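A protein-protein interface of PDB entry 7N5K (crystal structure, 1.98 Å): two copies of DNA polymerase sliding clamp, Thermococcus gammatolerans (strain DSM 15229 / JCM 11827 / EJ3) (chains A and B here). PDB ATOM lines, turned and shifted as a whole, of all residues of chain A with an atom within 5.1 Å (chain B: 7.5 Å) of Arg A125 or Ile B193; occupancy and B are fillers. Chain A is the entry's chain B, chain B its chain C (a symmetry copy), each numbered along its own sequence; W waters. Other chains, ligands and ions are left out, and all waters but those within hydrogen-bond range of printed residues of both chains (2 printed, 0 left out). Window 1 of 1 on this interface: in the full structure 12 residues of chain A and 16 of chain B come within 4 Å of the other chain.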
ATOM      1  N   ARG A  98      21.278 -13.168  21.982  1.00  0.00           N
ATOM      2  CA  ARG A  98      21.482 -13.951  20.769  1.00  0.00           C
ATOM      3  C   ARG A  98      20.314 -14.883  20.450  1.00  0.00           C
ATOM      4  O   ARG A  98      20.299 -15.466  19.367  1.00  0.00           O
ATOM      5  CB  ARG A  98      22.766 -14.779  20.884  1.00  0.00           C
ATOM      6  CG  ARG A  98      24.055 -13.975  21.194  1.00  0.00           C
ATOM      7  CD  ARG A  98      24.432 -12.909  20.135  1.00  0.00           C
ATOM      8  NE  ARG A  98      23.811 -13.044  18.814  1.00  0.00           N
ATOM      9  CZ  ARG A  98      23.069 -12.088  18.257  1.00  0.00           C
ATOM     10  NH1 ARG A  98      22.871 -10.943  18.903  1.00  0.00           N
ATOM     11  NH2 ARG A  98      22.530 -12.263  17.064  1.00  0.00           N
ATOM     12  N   GLY A  99      19.348 -15.056  21.355  1.00  0.00           N
ATOM     13  CA  GLY A  99      18.248 -15.960  21.081  1.00  0.00           C
ATOM     14  C   GLY A  99      17.251 -15.349  20.115  1.00  0.00           C
ATOM     15  O   GLY A  99      17.017 -14.146  20.115  1.00  0.00           O
ATOM     16  N   LYS A 100      16.661 -16.195  19.278  1.00  0.00           N
ATOM     17  CA  LYS A 100      15.652 -15.755  18.323  1.00  0.00           C
ATOM     18  C   LYS A 100      14.248 -16.002  18.864  1.00  0.00           C
ATOM     19  O   LYS A 100      14.035 -16.809  19.775  1.00  0.00           O
ATOM     20  CB  LYS A 100      15.826 -16.460  16.974  1.00  0.00           C
ATOM     21  CG  LYS A 100      17.245 -16.418  16.422  1.00  0.00           C
ATOM     22  CD  LYS A 100      17.809 -14.998  16.404  1.00  0.00           C
ATOM     23  CE  LYS A 100      19.309 -15.010  16.096  1.00  0.00           C
ATOM     24  NZ  LYS A 100      19.922 -13.640  16.057  1.00  0.00           N
ATOM     25  N   ASP A 103      13.343 -19.544  18.759  1.00  0.00           N
ATOM     26  CA  ASP A 103      14.205 -20.494  19.462  1.00  0.00           C
ATOM     27  C   ASP A 103      13.538 -21.035  20.720  1.00  0.00           C
ATOM     28  O   ASP A 103      12.860 -20.310  21.451  1.00  0.00           O
ATOM     29  CB  ASP A 103      15.527 -19.834  19.870  1.00  0.00           C
ATOM     30  CG  ASP A 103      16.488 -19.704  18.720  1.00  0.00           C
ATOM     31  OD1 ASP A 103      16.384 -20.504  17.760  1.00  0.00           O
ATOM     32  OD2 ASP A 103      17.344 -18.802  18.770  1.00  0.00           O
ATOM     33  N   ILE A 117      23.497 -22.534  28.419  1.00  0.00           N
ATOM     34  CA  ILE A 117      22.405 -21.805  27.790  1.00  0.00           C
ATOM     35  C   ILE A 117      22.360 -22.241  26.341  1.00  0.00           C
ATOM     36  O   ILE A 117      23.292 -21.949  25.571  1.00  0.00           O
ATOM     37  CB  ILE A 117      22.585 -20.283  27.893  1.00  0.00           C
ATOM     38  CG1 ILE A 117      22.659 -19.849  29.360  1.00  0.00           C
ATOM     39  CG2 ILE A 117      21.445 -19.560  27.151  1.00  0.00           C
ATOM     40  CD1 ILE A 117      23.274 -18.446  29.546  1.00  0.00           C
ATOM     41  N   THR A 118      21.278 -22.928  25.958  1.00  0.00           N
ATOM     42  CA  THR A 118      21.137 -23.479  24.618  1.00  0.00           C
ATOM     43  C   THR A 118      19.937 -22.856  23.911  1.00  0.00           C
ATOM     44  O   THR A 118      18.850 -22.734  24.495  1.00  0.00           O
ATOM     45  CB  THR A 118      20.994 -25.009  24.684  1.00  0.00           C
ATOM     46  OG1 THR A 118      22.134 -25.561  25.353  1.00  0.00           O
ATOM     47  CG2 THR A 118      20.895 -25.615  23.292  1.00  0.00           C
ATOM     48  N   PHE A 119      20.141 -22.472  22.655  1.00  0.00           N
ATOM     49  CA  PHE A 119      19.078 -22.052  21.762  1.00  0.00           C
ATOM     50  C   PHE A 119      18.883 -23.142  20.714  1.00  0.00           C
ATOM     51  O   PHE A 119      19.817 -23.461  19.967  1.00  0.00           O
ATOM     52  CB  PHE A 119      19.424 -20.736  21.083  1.00  0.00           C
ATOM     53  CG  PHE A 119      19.827 -19.643  22.032  1.00  0.00           C
ATOM     54  CD1 PHE A 119      18.922 -19.138  22.959  1.00  0.00           C
ATOM     55  CD2 PHE A 119      21.103 -19.104  21.983  1.00  0.00           C
ATOM     56  CE1 PHE A 119      19.288 -18.107  23.826  1.00  0.00           C
ATOM     57  CE2 PHE A 119      21.472 -18.075  22.849  1.00  0.00           C
ATOM     58  CZ  PHE A 119      20.567 -17.585  23.772  1.00  0.00           C
ATOM     59  N   ALA A 123      19.361 -24.235  14.299  1.00  0.00           N
ATOM     60  CA  ALA A 123      20.519 -25.000  14.721  1.00  0.00           C
ATOM     61  C   ALA A 123      20.466 -25.101  16.235  1.00  0.00           C
ATOM     62  O   ALA A 123      19.564 -24.555  16.882  1.00  0.00           O
ATOM     63  CB  ALA A 123      21.824 -24.339  14.251  1.00  0.00           C
ATOM     64  N   LYS A 124      21.447 -25.804  16.790  1.00  0.00           N
ATOM     65  CA  LYS A 124      21.650 -25.897  18.227  1.00  0.00           C
ATOM     66  C   LYS A 124      22.865 -25.051  18.599  1.00  0.00           C
ATOM     67  O   LYS A 124      23.981 -25.320  18.139  1.00  0.00           O
ATOM     68  CB  LYS A 124      21.840 -27.354  18.639  1.00  0.00           C
ATOM     69  CG  LYS A 124      21.827 -27.603  20.131  1.00  0.00           C
ATOM     70  CD  LYS A 124      22.426 -28.974  20.429  1.00  0.00           C
ATOM     71  CE  LYS A 124      22.348 -29.317  21.898  1.00  0.00           C
ATOM     72  NZ  LYS A 124      23.271 -30.429  22.272  1.00  0.00           N
ATOM     73  N   ARG A 125      22.643 -24.030  19.420  1.00  0.00           N
ATOM     74  CA  ARG A 125      23.688 -23.095  19.813  1.00  0.00           C
ATOM     75  C   ARG A 125      23.789 -23.120  21.329  1.00  0.00           C
ATOM     76  O   ARG A 125      22.812 -22.820  22.026  1.00  0.00           O
ATOM     77  CB  ARG A 125      23.385 -21.690  19.295  1.00  0.00           C
ATOM     78  CG  ARG A 125      23.231 -21.646  17.785  1.00  0.00           C
ATOM     79  CD  ARG A 125      22.949 -20.247  17.296  1.00  0.00           C
ATOM     80  NE  ARG A 125      21.624 -19.795  17.692  1.00  0.00           N
ATOM     81  CZ  ARG A 125      21.346 -18.573  18.143  1.00  0.00           C
ATOM     82  NH1 ARG A 125      22.304 -17.663  18.268  1.00  0.00           N
ATOM     83  NH2 ARG A 125      20.101 -18.259  18.467  1.00  0.00           N
ATOM     84  N   THR A 126      24.962 -23.487  21.835  1.00  0.00           N
ATOM     85  CA  THR A 126      25.156 -23.721  23.258  1.00  0.00           C
ATOM     86  C   THR A 126      26.251 -22.802  23.770  1.00  0.00           C
ATOM     87  O   THR A 126      27.391 -22.870  23.298  1.00  0.00           O
ATOM     88  CB  THR A 126      25.523 -25.183  23.526  1.00  0.00           C
ATOM     89  OG1 THR A 126      24.447 -26.033  23.114  1.00  0.00           O
ATOM     90  CG2 THR A 126      25.783 -25.405  25.003  1.00  0.00           C
ATOM     91  N   PHE A 127      25.904 -21.954  24.735  1.00  0.00           N
ATOM     92  CA  PHE A 127      26.851 -21.090  25.421  1.00  0.00           C
ATOM     93  C   PHE A 127      27.089 -21.597  26.835  1.00  0.00           C
ATOM     94  O   PHE A 127      26.185 -22.123  27.489  1.00  0.00           O
ATOM     95  CB  PHE A 127      26.355 -19.649  25.536  1.00  0.00           C
ATOM     96  CG  PHE A 127      26.154 -18.942  24.230  1.00  0.00           C
ATOM     97  CD1 PHE A 127      25.100 -19.270  23.403  1.00  0.00           C
ATOM     98  CD2 PHE A 127      26.988 -17.889  23.870  1.00  0.00           C
ATOM     99  CE1 PHE A 127      24.891 -18.580  22.211  1.00  0.00           C
ATOM    100  CE2 PHE A 127      26.789 -17.202  22.683  1.00  0.00           C
ATOM    101  CZ  PHE A 127      25.735 -17.550  21.854  1.00  0.00           C
ATOM    102  N   LEU B 152      24.508 -24.470   4.103  1.00  0.00           N
ATOM    103  CA  LEU B 152      23.731 -24.053   5.256  1.00  0.00           C
ATOM    104  C   LEU B 152      23.101 -22.703   4.978  1.00  0.00           C
ATOM    105  O   LEU B 152      23.531 -21.959   4.091  1.00  0.00           O
ATOM    106  CB  LEU B 152      24.583 -24.016   6.533  1.00  0.00           C
ATOM    107  CG  LEU B 152      25.588 -22.891   6.792  1.00  0.00           C
ATOM    108  CD1 LEU B 152      26.285 -23.176   8.114  1.00  0.00           C
ATOM    109  CD2 LEU B 152      26.640 -22.740   5.691  1.00  0.00           C
ATOM    110  N   GLU B 155      21.568 -17.345   7.663  1.00  0.00           N
ATOM    111  CA  GLU B 155      21.337 -16.861   9.024  1.00  0.00           C
ATOM    112  C   GLU B 155      22.021 -17.736  10.067  1.00  0.00           C
ATOM    113  O   GLU B 155      22.427 -17.229  11.116  1.00  0.00           O
ATOM    114  CB  GLU B 155      19.842 -16.745   9.317  1.00  0.00           C
ATOM    115  CG  GLU B 155      19.145 -18.075   9.407  1.00  0.00           C
ATOM    116  CD  GLU B 155      19.036 -18.559  10.836  1.00  0.00           C
ATOM    117  OE1 GLU B 155      19.483 -17.828  11.734  1.00  0.00           O
ATOM    118  OE2 GLU B 155      18.528 -19.678  11.055  1.00  0.00           O
ATOM    119  N   VAL B 156      22.163 -19.044   9.816  1.00  0.00           N
ATOM    120  CA  VAL B 156      22.913 -19.879  10.754  1.00  0.00           C
ATOM    121  C   VAL B 156      24.377 -19.462  10.778  1.00  0.00           C
ATOM    122  O   VAL B 156      24.993 -19.326  11.845  1.00  0.00           O
ATOM    123  CB  VAL B 156      22.777 -21.376  10.411  1.00  0.00           C
ATOM    124  CG1 VAL B 156      23.633 -22.203  11.369  1.00  0.00           C
ATOM    125  CG2 VAL B 156      21.349 -21.817  10.507  1.00  0.00           C
ATOM    126  N   LEU B 157      24.949 -19.243   9.596  1.00  0.00           N
ATOM    127  CA  LEU B 157      26.359 -18.887   9.490  1.00  0.00           C
ATOM    128  C   LEU B 157      26.625 -17.524  10.122  1.00  0.00           C
ATOM    129  O   LEU B 157      27.552 -17.362  10.922  1.00  0.00           O
ATOM    130  CB  LEU B 157      26.762 -18.896   8.018  1.00  0.00           C
ATOM    131  CG  LEU B 157      28.214 -18.604   7.670  1.00  0.00           C
ATOM    132  CD1 LEU B 157      29.148 -19.536   8.420  1.00  0.00           C
ATOM    133  CD2 LEU B 157      28.404 -18.694   6.156  1.00  0.00           C
ATOM    134  N   GLU B 159      24.831 -15.932  12.353  1.00  0.00           N
ATOM    135  CA  GLU B 159      24.599 -15.938  13.793  1.00  0.00           C
ATOM    136  C   GLU B 159      25.729 -16.647  14.526  1.00  0.00           C
ATOM    137  O   GLU B 159      26.178 -16.189  15.582  1.00  0.00           O
ATOM    138  CB  GLU B 159      23.246 -16.597  14.078  1.00  0.00           C
ATOM    139  CG  GLU B 159      22.713 -16.394  15.468  1.00  0.00           C
ATOM    140  CD  GLU B 159      22.766 -14.949  15.923  1.00  0.00           C
ATOM    141  OE1 GLU B 159      23.311 -14.703  17.018  1.00  0.00           O
ATOM    142  OE2 GLU B 159      22.262 -14.052  15.203  1.00  0.00           O
ATOM    143  N   ALA B 160      26.218 -17.758  13.967  1.00  0.00           N
ATOM    144  CA  ALA B 160      27.348 -18.453  14.575  1.00  0.00           C
ATOM    145  C   ALA B 160      28.565 -17.537  14.678  1.00  0.00           C
ATOM    146  O   ALA B 160      29.274 -17.537  15.690  1.00  0.00           O
ATOM    147  CB  ALA B 160      27.687 -19.710  13.767  1.00  0.00           C
ATOM    148  N   ILE B 161      28.804 -16.720  13.657  1.00  0.00           N
ATOM    149  CA  ILE B 161      29.982 -15.859  13.697  1.00  0.00           C
ATOM    150  C   ILE B 161      29.800 -14.745  14.731  1.00  0.00           C
ATOM    151  O   ILE B 161      30.711 -14.457  15.517  1.00  0.00           O
ATOM    152  CB  ILE B 161      30.274 -15.328  12.287  1.00  0.00           C
ATOM    153  CG1 ILE B 161      30.791 -16.505  11.443  1.00  0.00           C
ATOM    154  CG2 ILE B 161      31.269 -14.113  12.323  1.00  0.00           C
ATOM    155  CD1 ILE B 161      30.579 -16.326   9.977  1.00  0.00           C
ATOM    156  N   LYS B 162      28.599 -14.163  14.800  1.00  0.00           N
ATOM    157  CA  LYS B 162      28.305 -13.200  15.861  1.00  0.00           C
ATOM    158  C   LYS B 162      28.407 -13.838  17.246  1.00  0.00           C
ATOM    159  O   LYS B 162      29.002 -13.256  18.161  1.00  0.00           O
ATOM    160  CB  LYS B 162      26.917 -12.593  15.641  1.00  0.00           C
ATOM    161  CG  LYS B 162      26.511 -11.551  16.672  1.00  0.00           C
ATOM    162  CD  LYS B 162      27.442 -10.343  16.624  1.00  0.00           C
ATOM    163  CE  LYS B 162      27.081  -9.305  17.671  1.00  0.00           C
ATOM    164  NZ  LYS B 162      27.503  -7.954  17.225  1.00  0.00           N
ATOM    165  N   ASP B 163      27.836 -15.036  17.417  1.00  0.00           N
ATOM    166  CA  ASP B 163      27.943 -15.774  18.677  1.00  0.00           C
ATOM    167  C   ASP B 163      29.396 -15.992  19.089  1.00  0.00           C
ATOM    168  O   ASP B 163      29.773 -15.763  20.248  1.00  0.00           O
ATOM    169  CB  ASP B 163      27.250 -17.140  18.542  1.00  0.00           C
ATOM    170  CG  ASP B 163      25.730 -17.032  18.380  1.00  0.00           C
ATOM    171  OD1 ASP B 163      25.180 -15.917  18.483  1.00  0.00           O
ATOM    172  OD2 ASP B 163      25.097 -18.073  18.126  1.00  0.00           O
ATOM    173  N   ALA B 164      30.215 -16.497  18.163  1.00  0.00           N
ATOM    174  CA  ALA B 164      31.607 -16.792  18.493  1.00  0.00           C
ATOM    175  C   ALA B 164      32.367 -15.526  18.853  1.00  0.00           C
ATOM    176  O   ALA B 164      33.243 -15.542  19.735  1.00  0.00           O
ATOM    177  CB  ALA B 164      32.277 -17.506  17.314  1.00  0.00           C
ATOM    178  N   LEU B 171      37.388 -19.058  15.171  1.00  0.00           N
ATOM    179  CA  LEU B 171      36.274 -19.989  15.105  1.00  0.00           C
ATOM    180  C   LEU B 171      36.774 -21.299  14.510  1.00  0.00           C
ATOM    181  O   LEU B 171      37.298 -21.313  13.390  1.00  0.00           O
ATOM    182  CB  LEU B 171      35.142 -19.411  14.247  1.00  0.00           C
ATOM    183  CG  LEU B 171      33.836 -20.217  14.204  1.00  0.00           C
ATOM    184  CD1 LEU B 171      33.348 -20.526  15.615  1.00  0.00           C
ATOM    185  CD2 LEU B 171      32.782 -19.437  13.407  1.00  0.00           C
ATOM    186  N   LYS B 172      36.590 -22.389  15.241  1.00  0.00           N
ATOM    187  CA  LYS B 172      37.013 -23.702  14.780  1.00  0.00           C
ATOM    188  C   LYS B 172      35.867 -24.376  14.044  1.00  0.00           C
ATOM    189  O   LYS B 172      34.746 -24.460  14.569  1.00  0.00           O
ATOM    190  CB  LYS B 172      37.473 -24.564  15.956  1.00  0.00           C
ATOM    191  CG  LYS B 172      38.652 -23.982  16.730  1.00  0.00           C
ATOM    192  CD  LYS B 172      38.906 -24.748  18.018  1.00  0.00           C
ATOM    193  CE  LYS B 172      38.195 -24.096  19.202  1.00  0.00           C
ATOM    194  NZ  LYS B 172      38.540 -22.645  19.381  1.00  0.00           N
ATOM    195  N   ILE B 174      34.470 -27.872  12.478  1.00  0.00           N
ATOM    196  CA  ILE B 174      34.659 -29.306  12.679  1.00  0.00           C
ATOM    197  C   ILE B 174      33.553 -30.044  11.948  1.00  0.00           C
ATOM    198  O   ILE B 174      32.373 -29.911  12.295  1.00  0.00           O
ATOM    199  CB  ILE B 174      34.668 -29.699  14.163  1.00  0.00           C
ATOM    200  CG1 ILE B 174      35.729 -28.897  14.927  1.00  0.00           C
ATOM    201  CG2 ILE B 174      34.934 -31.186  14.298  1.00  0.00           C
ATOM    202  CD1 ILE B 174      35.365 -28.627  16.381  1.00  0.00           C
ATOM    203  N   PHE B 180      28.137 -31.013  11.765  1.00  0.00           N
ATOM    204  CA  PHE B 180      29.022 -29.887  11.499  1.00  0.00           C
ATOM    205  C   PHE B 180      28.952 -28.992  12.723  1.00  0.00           C
ATOM    206  O   PHE B 180      27.851 -28.641  13.166  1.00  0.00           O
ATOM    207  CB  PHE B 180      28.598 -29.120  10.230  1.00  0.00           C
ATOM    208  CG  PHE B 180      29.359 -27.831   9.999  1.00  0.00           C
ATOM    209  CD1 PHE B 180      30.727 -27.841   9.756  1.00  0.00           C
ATOM    210  CD2 PHE B 180      28.700 -26.617  10.007  1.00  0.00           C
ATOM    211  CE1 PHE B 180      31.425 -26.651   9.542  1.00  0.00           C
ATOM    212  CE2 PHE B 180      29.380 -25.428   9.786  1.00  0.00           C
ATOM    213  CZ  PHE B 180      30.752 -25.445   9.558  1.00  0.00           C
ATOM    214  N   THR B 181      30.115 -28.671  13.298  1.00  0.00           N
ATOM    215  CA  THR B 181      30.190 -27.877  14.520  1.00  0.00           C
ATOM    216  C   THR B 181      31.113 -26.691  14.287  1.00  0.00           C
ATOM    217  O   THR B 181      32.192 -26.849  13.704  1.00  0.00           O
ATOM    218  CB  THR B 181      30.699 -28.717  15.698  1.00  0.00           C
ATOM    219  OG1 THR B 181      29.774 -29.777  15.964  1.00  0.00           O
ATOM    220  CG2 THR B 181      30.825 -27.869  16.938  1.00  0.00           C
ATOM    221  N   MET B 182      30.677 -25.504  14.710  1.00  0.00           N
ATOM    222  CA  MET B 182      31.535 -24.330  14.800  1.00  0.00           C
ATOM    223  C   MET B 182      31.694 -24.022  16.282  1.00  0.00           C
ATOM    224  O   MET B 182      30.695 -23.869  16.993  1.00  0.00           O
ATOM    225  CB  MET B 182      30.942 -23.144  14.039  1.00  0.00           C
ATOM    226  CG  MET B 182      30.869 -23.381  12.539  1.00  0.00           C
ATOM    227  SD  MET B 182      29.886 -22.206  11.589  1.00  0.00           S
ATOM    228  CE  MET B 182      28.219 -22.757  12.039  1.00  0.00           C
ATOM    229  N   LYS B 183      32.940 -23.982  16.752  1.00  0.00           N
ATOM    230  CA  LYS B 183      33.227 -23.865  18.178  1.00  0.00           C
ATOM    231  C   LYS B 183      34.242 -22.760  18.421  1.00  0.00           C
ATOM    232  O   LYS B 183      35.213 -22.599  17.666  1.00  0.00           O
ATOM    233  CB  LYS B 183      33.757 -25.198  18.764  1.00  0.00           C
ATOM    234  CG  LYS B 183      34.208 -25.098  20.214  1.00  0.00           C
ATOM    235  CD  LYS B 183      35.087 -26.274  20.618  1.00  0.00           C
ATOM    236  CE  LYS B 183      34.258 -27.486  21.003  1.00  0.00           C
ATOM    237  NZ  LYS B 183      34.773 -28.132  22.247  1.00  0.00           N
ATOM    238  N   ALA B 184      34.010 -22.002  19.488  1.00  0.00           N
ATOM    239  CA  ALA B 184      34.918 -20.949  19.904  1.00  0.00           C
ATOM    240  C   ALA B 184      35.031 -20.980  21.416  1.00  0.00           C
ATOM    241  O   ALA B 184      34.048 -21.251  22.115  1.00  0.00           O
ATOM    242  CB  ALA B 184      34.446 -19.578  19.436  1.00  0.00           C
ATOM    243  N   GLU B 190      32.649 -20.193  26.338  1.00  0.00           N
ATOM    244  CA  GLU B 190      32.691 -21.079  25.186  1.00  0.00           C
ATOM    245  C   GLU B 190      31.320 -21.104  24.519  1.00  0.00           C
ATOM    246  O   GLU B 190      30.287 -20.967  25.179  1.00  0.00           O
ATOM    247  CB  GLU B 190      33.113 -22.498  25.591  1.00  0.00           C
ATOM    248  CG  GLU B 190      33.597 -23.358  24.434  1.00  0.00           C
ATOM    249  CD  GLU B 190      32.692 -24.545  24.160  1.00  0.00           C
ATOM    250  OE1 GLU B 190      31.483 -24.466  24.472  1.00  0.00           O
ATOM    251  OE2 GLU B 190      33.197 -25.556  23.630  1.00  0.00           O
ATOM    252  N   VAL B 191      31.323 -21.274  23.202  1.00  0.00           N
ATOM    253  CA  VAL B 191      30.094 -21.437  22.442  1.00  0.00           C
ATOM    254  C   VAL B 191      30.358 -22.487  21.383  1.00  0.00           C
ATOM    255  O   VAL B 191      31.468 -22.585  20.845  1.00  0.00           O
ATOM    256  CB  VAL B 191      29.570 -20.116  21.827  1.00  0.00           C
ATOM    257  CG1 VAL B 191      30.467 -19.608  20.723  1.00  0.00           C
ATOM    258  CG2 VAL B 191      28.124 -20.303  21.300  1.00  0.00           C
ATOM    259  N   GLU B 192      29.340 -23.303  21.135  1.00  0.00           N
ATOM    260  CA  GLU B 192      29.345 -24.301  20.083  1.00  0.00           C
ATOM    261  C   GLU B 192      28.049 -24.160  19.304  1.00  0.00           C
ATOM    262  O   GLU B 192      26.971 -24.120  19.904  1.00  0.00           O
ATOM    263  CB  GLU B 192      29.451 -25.710  20.674  1.00  0.00           C
ATOM    264  CG  GLU B 192      30.675 -25.935  21.545  1.00  0.00           C
ATOM    265  CD  GLU B 192      30.655 -27.300  22.214  1.00  0.00           C
ATOM    266  OE1 GLU B 192      31.499 -27.547  23.109  1.00  0.00           O
ATOM    267  OE2 GLU B 192      29.791 -28.123  21.841  1.00  0.00           O
ATOM    268  N   ILE B 193      28.148 -24.072  17.983  1.00  0.00           N
ATOM    269  CA  ILE B 193      26.981 -24.131  17.106  1.00  0.00           C
ATOM    270  C   ILE B 193      27.046 -25.471  16.391  1.00  0.00           C
ATOM    271  O   ILE B 193      28.017 -25.741  15.671  1.00  0.00           O
ATOM    272  CB  ILE B 193      26.948 -22.959  16.114  1.00  0.00           C
ATOM    273  CG1 ILE B 193      26.958 -21.626  16.871  1.00  0.00           C
ATOM    274  CG2 ILE B 193      25.713 -23.062  15.175  1.00  0.00           C
ATOM    275  CD1 ILE B 193      28.368 -21.026  17.077  1.00  0.00           C
ATOM    276  N   LYS B 194      26.039 -26.317  16.606  1.00  0.00           N
ATOM    277  CA  LYS B 194      25.994 -27.662  16.037  1.00  0.00           C
ATOM    278  C   LYS B 194      24.844 -27.824  15.044  1.00  0.00           C
ATOM    279  O   LYS B 194      23.711 -27.408  15.306  1.00  0.00           O
ATOM    280  CB  LYS B 194      25.863 -28.720  17.132  1.00  0.00           C
ATOM    281  CG  LYS B 194      26.712 -28.432  18.362  1.00  0.00           C
ATOM    282  CD  LYS B 194      27.106 -29.717  19.085  1.00  0.00           C
ATOM    283  CE  LYS B 194      27.343 -29.473  20.573  1.00  0.00           C
ATOM    284  NZ  LYS B 194      26.216 -29.969  21.428  1.00  0.00           N
ATOM    285  N   LEU B 195      25.146 -28.457  13.909  1.00  0.00           N
ATOM    286  CA  LEU B 195      24.178 -28.725  12.857  1.00  0.00           C
ATOM    287  C   LEU B 195      24.220 -30.202  12.477  1.00  0.00           C
ATOM    288  O   LEU B 195      25.299 -30.760  12.248  1.00  0.00           O
ATOM    289  CB  LEU B 195      24.463 -27.867  11.624  1.00  0.00           C
ATOM    290  CG  LEU B 195      23.982 -26.420  11.674  1.00  0.00           C
ATOM    291  CD1 LEU B 195      24.689 -25.593  10.628  1.00  0.00           C
ATOM    292  CD2 LEU B 195      22.480 -26.378  11.457  1.00  0.00           C
HETATM  293  O   HOH W   1      25.341 -26.943  20.696  1.00  0.00           O
HETATM  294  O   HOH W   2      29.096 -25.141  24.497  1.00  0.00           O
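The side-chain carboxylate of Asp B163 lies within salt-bridge range of the guanidinium group of Arg A125, 2.8 Å away.
N of Lys B194 lies within hydrogen-bond range of O of Lys A124.
The guanidinium group of Arg A125 is in salt-bridge range of the side-chain carboxylate of Glu B159, at 3.4 Å.
The guanidinium group of Arg A98 lies within salt-bridge range of the side-chain carboxylate of Glu B159 (2.5 Å).
The backbone NH (N) of Thr A126 sits at hydrogen-bond distance from the backbone carbonyl oxygen (O) of Glu B192 (2.9 Å).
The side-chain amino group (NZ) of Lys A100 lies within salt-bridge range of the side-chain carboxylate (OE2) of Glu B159 (2.5 Å).
NE of Arg A98 is in salt-bridge range of OD1 of Asp B163.
The side-chain hydroxyl of Thr A118 lies within hydrogen-bond range of the side-chain hydroxyl of Thr A126, 3.3 Å away.
N of Leu B195 lies within hydrogen-bond range of O of Phe B180, 2.8 Å away.
The side-chain carboxylate (OE2) of Glu B190 sits close to the side-chain carboxylate (OE1) of Glu B192, at 2.7 Å.
OE2 of Glu B190 is in salt-bridge range of NZ of Lys B183.
The side-chain amino group (NZ) of Lys B183 lies within salt-bridge range of the side-chain carboxylate (OE1) of Glu B192, at 3.4 Å.
The guanidinium group (NH2) of Arg A125 is in hydrogen-bond range of the backbone carbonyl oxygen (O) of Arg A98 (2.9 Å).
No position is printed for both chains.
Of the 19 pairs that touch across the chains among the printed residues, none has its exchanged pair printed and touching as well.
Arg A98 touches Lys B162.
Lys B194 touches Ala A123.
Leu B195 touches Ala A123.
Lys A124 touches Glu B192.
CA of Arg A125 touches O of Glu B192, 3.4 Å away.
Ile B193 touches Arg A125.
Thr A126 touches Glu B190 (O to O, 3.9 Å).
Thr A126 touches Val B191 (O to CA, 3.2 Å).
Asp B163 touches Phe A127.
Glu B190 touches Phe A127 (O to CA, 3.4 Å).
Of the printed residues of chain B, Lys A100 touches Glu B159.
Of the printed residues of chain A, Glu B159 touches Arg A98 (2.5 Å), Lys A100 (2.5 Å) and Arg A125 (3.1 Å).
Printed residues of chain B within 4 Å of Lys A124: Glu B192, Ile B193 and Lys B194.
Of the printed residues of chain A, Lys B194 touches Ala A123 and Lys A124.
Gly A99 touches none of the printed residues of chain B.
The nearest residue of chain A that does not touch Ile B193 is Ala A123 (4.2 Å).
The nearest printed residue of chain B that does not touch Arg A98 is Ala B164 (7.1 Å).
Water W2 lies within hydrogen-bond range of the side-chain carboxylate (OE1) of Glu B190 (2.5 Å) and the backbone carbonyl oxygen (O) of Thr A126 (3.1 Å).
Water W1 lies within hydrogen-bond range of OG1 of Thr A126, NZ of Lys B194, O of Lys A124 and O of Glu B192.
Of the 24 printed residues of chain B, 9 touch a printed residue of chain A.
Hydrophobic or aromatic side chains of chain B within 4 Å of the printed part of chain A: Val B191, Ile B193 and Leu B195.
Among the printed residues, 19 pairs touch across the chains.
Among the printed residues, Asp or Glu carboxylates within 4 Å of a Lys or Arg side-chain nitrogen of the other chain: Arg A98 with Glu B159, Arg A98 with Asp B163, Lys A100 with Glu B159, Arg A125 with Glu B159 and Arg A125 with Asp B163.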
